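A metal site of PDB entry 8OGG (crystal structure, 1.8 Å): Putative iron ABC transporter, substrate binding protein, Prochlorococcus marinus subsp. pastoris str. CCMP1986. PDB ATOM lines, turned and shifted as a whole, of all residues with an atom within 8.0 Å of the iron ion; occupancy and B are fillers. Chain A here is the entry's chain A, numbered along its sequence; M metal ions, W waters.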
ATOM      1  N   GLY A  10       7.043  18.228 -18.553  1.00  0.00           N
ATOM      2  CA  GLY A  10       8.473  18.030 -18.263  1.00  0.00           C
ATOM      3  C   GLY A  10       8.856  18.529 -16.878  1.00  0.00           C
ATOM      4  O   GLY A  10      10.054  18.418 -16.549  1.00  0.00           O
ATOM      5  N   ARG A  11       7.891  19.052 -16.104  1.00  0.00           N
ATOM      6  CA  ARG A  11       8.101  19.512 -14.706  1.00  0.00           C
ATOM      7  C   ARG A  11       8.161  18.265 -13.827  1.00  0.00           C
ATOM      8  O   ARG A  11       7.132  17.886 -13.216  1.00  0.00           O
ATOM      9  CB  ARG A  11       7.005  20.468 -14.224  1.00  0.00           C
ATOM     10  CG  ARG A  11       7.257  21.927 -14.573  1.00  0.00           C
ATOM     11  CD  ARG A  11       6.076  22.813 -14.185  1.00  0.00           C
ATOM     12  NE  ARG A  11       5.803  22.755 -12.747  1.00  0.00           N
ATOM     13  CZ  ARG A  11       6.469  23.446 -11.830  1.00  0.00           C
ATOM     14  NH1 ARG A  11       7.446  24.259 -12.191  1.00  0.00           N
ATOM     15  NH2 ARG A  11       6.171  23.328 -10.553  1.00  0.00           N
ATOM     16  N   HIS A  12       9.327  17.624 -13.827  1.00  0.00           N
ATOM     17  CA  HIS A  12       9.547  16.259 -13.291  1.00  0.00           C
ATOM     18  C   HIS A  12      10.048  16.368 -11.850  1.00  0.00           C
ATOM     19  O   HIS A  12      11.180  15.935 -11.546  1.00  0.00           O
ATOM     20  CB  HIS A  12      10.480  15.503 -14.252  1.00  0.00           C
ATOM     21  CG  HIS A  12      10.450  14.028 -14.053  1.00  0.00           C
ATOM     22  ND1 HIS A  12      11.425  13.194 -14.593  1.00  0.00           N
ATOM     23  CD2 HIS A  12       9.607  13.246 -13.355  1.00  0.00           C
ATOM     24  CE1 HIS A  12      11.143  11.941 -14.259  1.00  0.00           C
ATOM     25  NE2 HIS A  12      10.046  11.948 -13.494  1.00  0.00           N
ATOM     26  N   TYR A  13       9.239  16.995 -10.985  1.00  0.00           N
ATOM     27  CA  TYR A  13       9.566  17.237  -9.554  1.00  0.00           C
ATOM     28  C   TYR A  13       8.616  16.420  -8.676  1.00  0.00           C
ATOM     29  O   TYR A  13       8.917  16.297  -7.486  1.00  0.00           O
ATOM     30  CB  TYR A  13       9.505  18.737  -9.280  1.00  0.00           C
ATOM     31  CG  TYR A  13      10.545  19.551 -10.025  1.00  0.00           C
ATOM     32  CD1 TYR A  13      11.891  19.518  -9.638  1.00  0.00           C
ATOM     33  CD2 TYR A  13      10.205  20.352 -11.099  1.00  0.00           C
ATOM     34  CE1 TYR A  13      12.852  20.271 -10.293  1.00  0.00           C
ATOM     35  CE2 TYR A  13      11.169  21.115 -11.763  1.00  0.00           C
ATOM     36  CZ  TYR A  13      12.495  21.079 -11.354  1.00  0.00           C
ATOM     37  OH  TYR A  13      13.446  21.822 -11.979  1.00  0.00           O
ATOM     38  N   VAL A  60      10.630  22.625 -19.080  1.00  0.00           N
ATOM     39  CA  VAL A  60      11.574  23.337 -18.170  1.00  0.00           C
ATOM     40  C   VAL A  60      12.782  23.774 -18.985  1.00  0.00           C
ATOM     41  O   VAL A  60      13.365  22.901 -19.662  1.00  0.00           O
ATOM     42  CB  VAL A  60      11.991  22.464 -16.983  1.00  0.00           C
ATOM     43  CG1 VAL A  60      12.923  23.212 -16.045  1.00  0.00           C
ATOM     44  CG2 VAL A  60      10.778  21.969 -16.228  1.00  0.00           C
ATOM     45  N   ASP A  61      13.063  25.084 -18.923  1.00  0.00           N
ATOM     46  CA  ASP A  61      14.270  25.800 -19.428  1.00  0.00           C
ATOM     47  C   ASP A  61      14.065  26.317 -20.859  1.00  0.00           C
ATOM     48  O   ASP A  61      13.584  25.576 -21.744  1.00  0.00           O
ATOM     49  CB  ASP A  61      15.565  24.983 -19.317  1.00  0.00           C
ATOM     50  CG  ASP A  61      16.835  25.842 -19.367  1.00  0.00           C
ATOM     51  OD1 ASP A  61      17.350  26.093 -20.483  1.00  0.00           O
ATOM     52  OD2 ASP A  61      17.303  26.267 -18.298  1.00  0.00           O
ATOM     53  N   ARG A 103      12.742  30.744 -12.258  1.00  0.00           N
ATOM     54  CA  ARG A 103      13.891  30.269 -11.453  1.00  0.00           C
ATOM     55  C   ARG A 103      15.082  31.192 -11.728  1.00  0.00           C
ATOM     56  O   ARG A 103      15.154  31.825 -12.815  1.00  0.00           O
ATOM     57  CB  ARG A 103      14.173  28.782 -11.719  1.00  0.00           C
ATOM     58  CG  ARG A 103      14.491  28.417 -13.170  1.00  0.00           C
ATOM     59  CD  ARG A 103      13.302  27.903 -13.970  1.00  0.00           C
ATOM     60  NE  ARG A 103      12.645  26.806 -13.283  1.00  0.00           N
ATOM     61  CZ  ARG A 103      13.110  25.551 -13.214  1.00  0.00           C
ATOM     62  NH1 ARG A 103      14.242  25.217 -13.812  1.00  0.00           N
ATOM     63  NH2 ARG A 103      12.427  24.656 -12.512  1.00  0.00           N
ATOM     64  N   ARG A 105      19.393  31.058 -11.664  1.00  0.00           N
ATOM     65  CA  ARG A 105      20.689  30.348 -11.516  1.00  0.00           C
ATOM     66  C   ARG A 105      21.632  31.291 -10.772  1.00  0.00           C
ATOM     67  O   ARG A 105      21.926  32.379 -11.277  1.00  0.00           O
ATOM     68  CB  ARG A 105      21.237  29.879 -12.857  1.00  0.00           C
ATOM     69  CG  ARG A 105      22.251  28.732 -12.760  1.00  0.00           C
ATOM     70  CD  ARG A 105      22.203  27.787 -13.929  1.00  0.00           C
ATOM     71  NE  ARG A 105      23.014  26.578 -13.799  1.00  0.00           N
ATOM     72  CZ  ARG A 105      22.676  25.473 -13.129  1.00  0.00           C
ATOM     73  NH1 ARG A 105      21.517  25.401 -12.493  1.00  0.00           N
ATOM     74  NH2 ARG A 105      23.501  24.439 -13.124  1.00  0.00           N
ATOM     75  N   ARG A 137      28.509  21.977 -12.521  1.00  0.00           N
ATOM     76  CA  ARG A 137      27.792  20.908 -13.240  1.00  0.00           C
ATOM     77  C   ARG A 137      28.223  20.960 -14.717  1.00  0.00           C
ATOM     78  O   ARG A 137      28.651  22.055 -15.185  1.00  0.00           O
ATOM     79  CB  ARG A 137      26.289  21.087 -13.035  1.00  0.00           C
ATOM     80  CG  ARG A 137      25.410  20.218 -13.927  1.00  0.00           C
ATOM     81  CD  ARG A 137      23.983  20.285 -13.453  1.00  0.00           C
ATOM     82  NE  ARG A 137      23.132  19.240 -13.990  1.00  0.00           N
ATOM     83  CZ  ARG A 137      21.835  19.122 -13.734  1.00  0.00           C
ATOM     84  NH1 ARG A 137      21.237  19.990 -12.945  1.00  0.00           N
ATOM     85  NH2 ARG A 137      21.151  18.116 -14.253  1.00  0.00           N
ATOM     86  N   SER A 141      23.827  20.083 -19.035  1.00  0.00           N
ATOM     87  CA  SER A 141      22.698  20.739 -18.334  1.00  0.00           C
ATOM     88  C   SER A 141      22.170  21.917 -19.142  1.00  0.00           C
ATOM     89  O   SER A 141      22.878  22.900 -19.334  1.00  0.00           O
ATOM     90  CB  SER A 141      23.086  21.201 -16.945  1.00  0.00           C
ATOM     91  OG  SER A 141      21.983  21.858 -16.349  1.00  0.00           O
ATOM     92  N   TYR A 143      20.371  24.225 -18.034  1.00  0.00           N
ATOM     93  CA  TYR A 143      20.519  25.345 -17.071  1.00  0.00           C
ATOM     94  C   TYR A 143      21.849  26.087 -17.340  1.00  0.00           C
ATOM     95  O   TYR A 143      21.860  27.318 -17.384  1.00  0.00           O
ATOM     96  CB  TYR A 143      20.455  24.848 -15.627  1.00  0.00           C
ATOM     97  CG  TYR A 143      19.209  24.102 -15.195  1.00  0.00           C
ATOM     98  CD1 TYR A 143      17.990  24.312 -15.821  1.00  0.00           C
ATOM     99  CD2 TYR A 143      19.244  23.206 -14.133  1.00  0.00           C
ATOM    100  CE1 TYR A 143      16.843  23.666 -15.414  1.00  0.00           C
ATOM    101  CE2 TYR A 143      18.102  22.526 -13.732  1.00  0.00           C
ATOM    102  CZ  TYR A 143      16.892  22.775 -14.352  1.00  0.00           C
ATOM    103  OH  TYR A 143      15.719  22.156 -13.968  1.00  0.00           O
ATOM    104  N   ASP A 179      22.562  19.431  -9.737  1.00  0.00           N
ATOM    105  CA  ASP A 179      22.679  20.661  -8.915  1.00  0.00           C
ATOM    106  C   ASP A 179      22.734  20.279  -7.425  1.00  0.00           C
ATOM    107  O   ASP A 179      23.431  20.948  -6.647  1.00  0.00           O
ATOM    108  CB  ASP A 179      21.523  21.638  -9.168  1.00  0.00           C
ATOM    109  CG  ASP A 179      21.707  22.575 -10.359  1.00  0.00           C
ATOM    110  OD1 ASP A 179      22.424  22.216 -11.312  1.00  0.00           O
ATOM    111  OD2 ASP A 179      21.156  23.668 -10.302  1.00  0.00           O
ATOM    112  N   ASN A 197      20.574  26.263  -9.403  1.00  0.00           N
ATOM    113  CA  ASN A 197      19.257  26.930  -9.372  1.00  0.00           C
ATOM    114  C   ASN A 197      18.876  27.135  -7.910  1.00  0.00           C
ATOM    115  O   ASN A 197      19.146  26.241  -7.098  1.00  0.00           O
ATOM    116  CB  ASN A 197      18.176  26.180 -10.141  1.00  0.00           C
ATOM    117  CG  ASN A 197      18.333  26.259 -11.654  1.00  0.00           C
ATOM    118  OD1 ASN A 197      19.073  27.083 -12.171  1.00  0.00           O
ATOM    119  ND2 ASN A 197      17.623  25.386 -12.352  1.00  0.00           N
ATOM    120  N   TYR A 199      16.090  27.123  -6.239  1.00  0.00           N
ATOM    121  CA  TYR A 199      15.013  26.280  -5.679  1.00  0.00           C
ATOM    122  C   TYR A 199      15.573  24.977  -5.098  1.00  0.00           C
ATOM    123  O   TYR A 199      14.961  24.513  -4.149  1.00  0.00           O
ATOM    124  CB  TYR A 199      13.852  26.065  -6.667  1.00  0.00           C
ATOM    125  CG  TYR A 199      14.236  25.367  -7.945  1.00  0.00           C
ATOM    126  CD1 TYR A 199      14.232  23.991  -8.039  1.00  0.00           C
ATOM    127  CD2 TYR A 199      14.614  26.109  -9.047  1.00  0.00           C
ATOM    128  CE1 TYR A 199      14.608  23.353  -9.215  1.00  0.00           C
ATOM    129  CE2 TYR A 199      15.008  25.485 -10.223  1.00  0.00           C
ATOM    130  CZ  TYR A 199      15.005  24.107 -10.306  1.00  0.00           C
ATOM    131  OH  TYR A 199      15.434  23.533 -11.478  1.00  0.00           O
ATOM    132  N   TYR A 200      16.694  24.436  -5.596  1.00  0.00           N
ATOM    133  CA  TYR A 200      17.357  23.220  -5.044  1.00  0.00           C
ATOM    134  C   TYR A 200      17.879  23.524  -3.624  1.00  0.00           C
ATOM    135  O   TYR A 200      17.681  22.663  -2.755  1.00  0.00           O
ATOM    136  CB  TYR A 200      18.464  22.699  -5.965  1.00  0.00           C
ATOM    137  CG  TYR A 200      17.961  22.187  -7.299  1.00  0.00           C
ATOM    138  CD1 TYR A 200      17.075  21.119  -7.367  1.00  0.00           C
ATOM    139  CD2 TYR A 200      18.324  22.810  -8.480  1.00  0.00           C
ATOM    140  CE1 TYR A 200      16.570  20.672  -8.577  1.00  0.00           C
ATOM    141  CE2 TYR A 200      17.832  22.370  -9.701  1.00  0.00           C
ATOM    142  CZ  TYR A 200      16.956  21.296  -9.761  1.00  0.00           C
ATOM    143  OH  TYR A 200      16.464  20.876 -10.968  1.00  0.00           O
ATOM    144  N   ARG A 203      14.721  23.619  -1.273  1.00  0.00           N
ATOM    145  CA  ARG A 203      14.180  22.252  -1.081  1.00  0.00           C
ATOM    146  C   ARG A 203      15.029  21.537  -0.018  1.00  0.00           C
ATOM    147  O   ARG A 203      14.465  20.910   0.879  1.00  0.00           O
ATOM    148  CB  ARG A 203      14.186  21.452  -2.386  1.00  0.00           C
ATOM    149  CG  ARG A 203      13.023  21.758  -3.319  1.00  0.00           C
ATOM    150  CD  ARG A 203      13.126  21.037  -4.662  1.00  0.00           C
ATOM    151  NE  ARG A 203      12.561  19.678  -4.741  1.00  0.00           N
ATOM    152  CZ  ARG A 203      11.252  19.367  -4.720  1.00  0.00           C
ATOM    153  NH1 ARG A 203      10.887  18.093  -4.838  1.00  0.00           N
ATOM    154  NH2 ARG A 203      10.317  20.291  -4.557  1.00  0.00           N
ATOM    155  N   THR A 233       9.813  27.819 -16.637  1.00  0.00           N
ATOM    156  CA  THR A 233       8.994  26.711 -17.147  1.00  0.00           C
ATOM    157  C   THR A 233       7.862  27.396 -17.909  1.00  0.00           C
ATOM    158  O   THR A 233       7.538  28.549 -17.571  1.00  0.00           O
ATOM    159  CB  THR A 233       8.569  25.743 -16.026  1.00  0.00           C
ATOM    160  OG1 THR A 233       7.473  26.291 -15.295  1.00  0.00           O
ATOM    161  CG2 THR A 233       9.696  25.418 -15.062  1.00  0.00           C
ATOM    162  N   THR A 267       7.547  23.896  -5.901  1.00  0.00           N
ATOM    163  CA  THR A 267       8.972  23.660  -6.260  1.00  0.00           C
ATOM    164  C   THR A 267       9.895  24.759  -5.712  1.00  0.00           C
ATOM    165  O   THR A 267      11.093  24.683  -6.009  1.00  0.00           O
ATOM    166  CB  THR A 267       9.142  23.531  -7.778  1.00  0.00           C
ATOM    167  OG1 THR A 267       8.601  24.714  -8.370  1.00  0.00           O
ATOM    168  CG2 THR A 267       8.470  22.314  -8.363  1.00  0.00           C
ATOM    169  N   GLU A 269       9.940  27.909  -6.452  1.00  0.00           N
ATOM    170  CA  GLU A 269      10.196  28.889  -7.543  1.00  0.00           C
ATOM    171  C   GLU A 269       9.490  30.207  -7.207  1.00  0.00           C
ATOM    172  O   GLU A 269       8.808  30.270  -6.163  1.00  0.00           O
ATOM    173  CB  GLU A 269       9.724  28.352  -8.894  1.00  0.00           C
ATOM    174  CG  GLU A 269      10.494  27.129  -9.364  1.00  0.00           C
ATOM    175  CD  GLU A 269      10.031  26.551 -10.682  1.00  0.00           C
ATOM    176  OE1 GLU A 269       9.365  25.509 -10.658  1.00  0.00           O
ATOM    177  OE2 GLU A 269      10.324  27.138 -11.729  1.00  0.00           O
HETATM  178 FE    FE M   1      15.243  21.737 -12.109  1.00  0.00          FE
HETATM  179  O   HOH W   1      14.850  19.605 -12.855  1.00  0.00           O
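OH of Tyr 13 binds the iron ion. OH of Tyr 200 binds the iron ion, at 1.9 Å. The side-chain hydroxyl (OH) of Tyr 199 is bound to the iron ion. The side-chain hydroxyl (OH) of Tyr 143 binds the iron ion (2.0 Å). Water W1 binds the iron ion.
The side-chain hydroxyl (OH) of Tyr 199 sits close to the guanidinium group (NH1) of Arg 103 (3.1 Å). The guanidinium group (NH2) of Arg 103 lies close to the side-chain hydroxyl (OH) of Tyr 13 (3.1 Å). NH1 of Arg 103 sits close to OH of Tyr 143, at 3.4 Å. The backbone NH of Tyr 143 lies close to the side-chain hydroxyl of Ser 141 (3.3 Å). OH of Tyr 199 sits close to ND2 of Asn 197.
Four residues have an atom within 4 Å of the iron ion: Tyr 13, Tyr 143, Tyr 199 and Tyr 200. Along chain A the residues within 4 Å of the iron ion span positions 13 to 200. The nearest printed residue that does not touch the iron ion is Arg 103 (4.002 Å).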
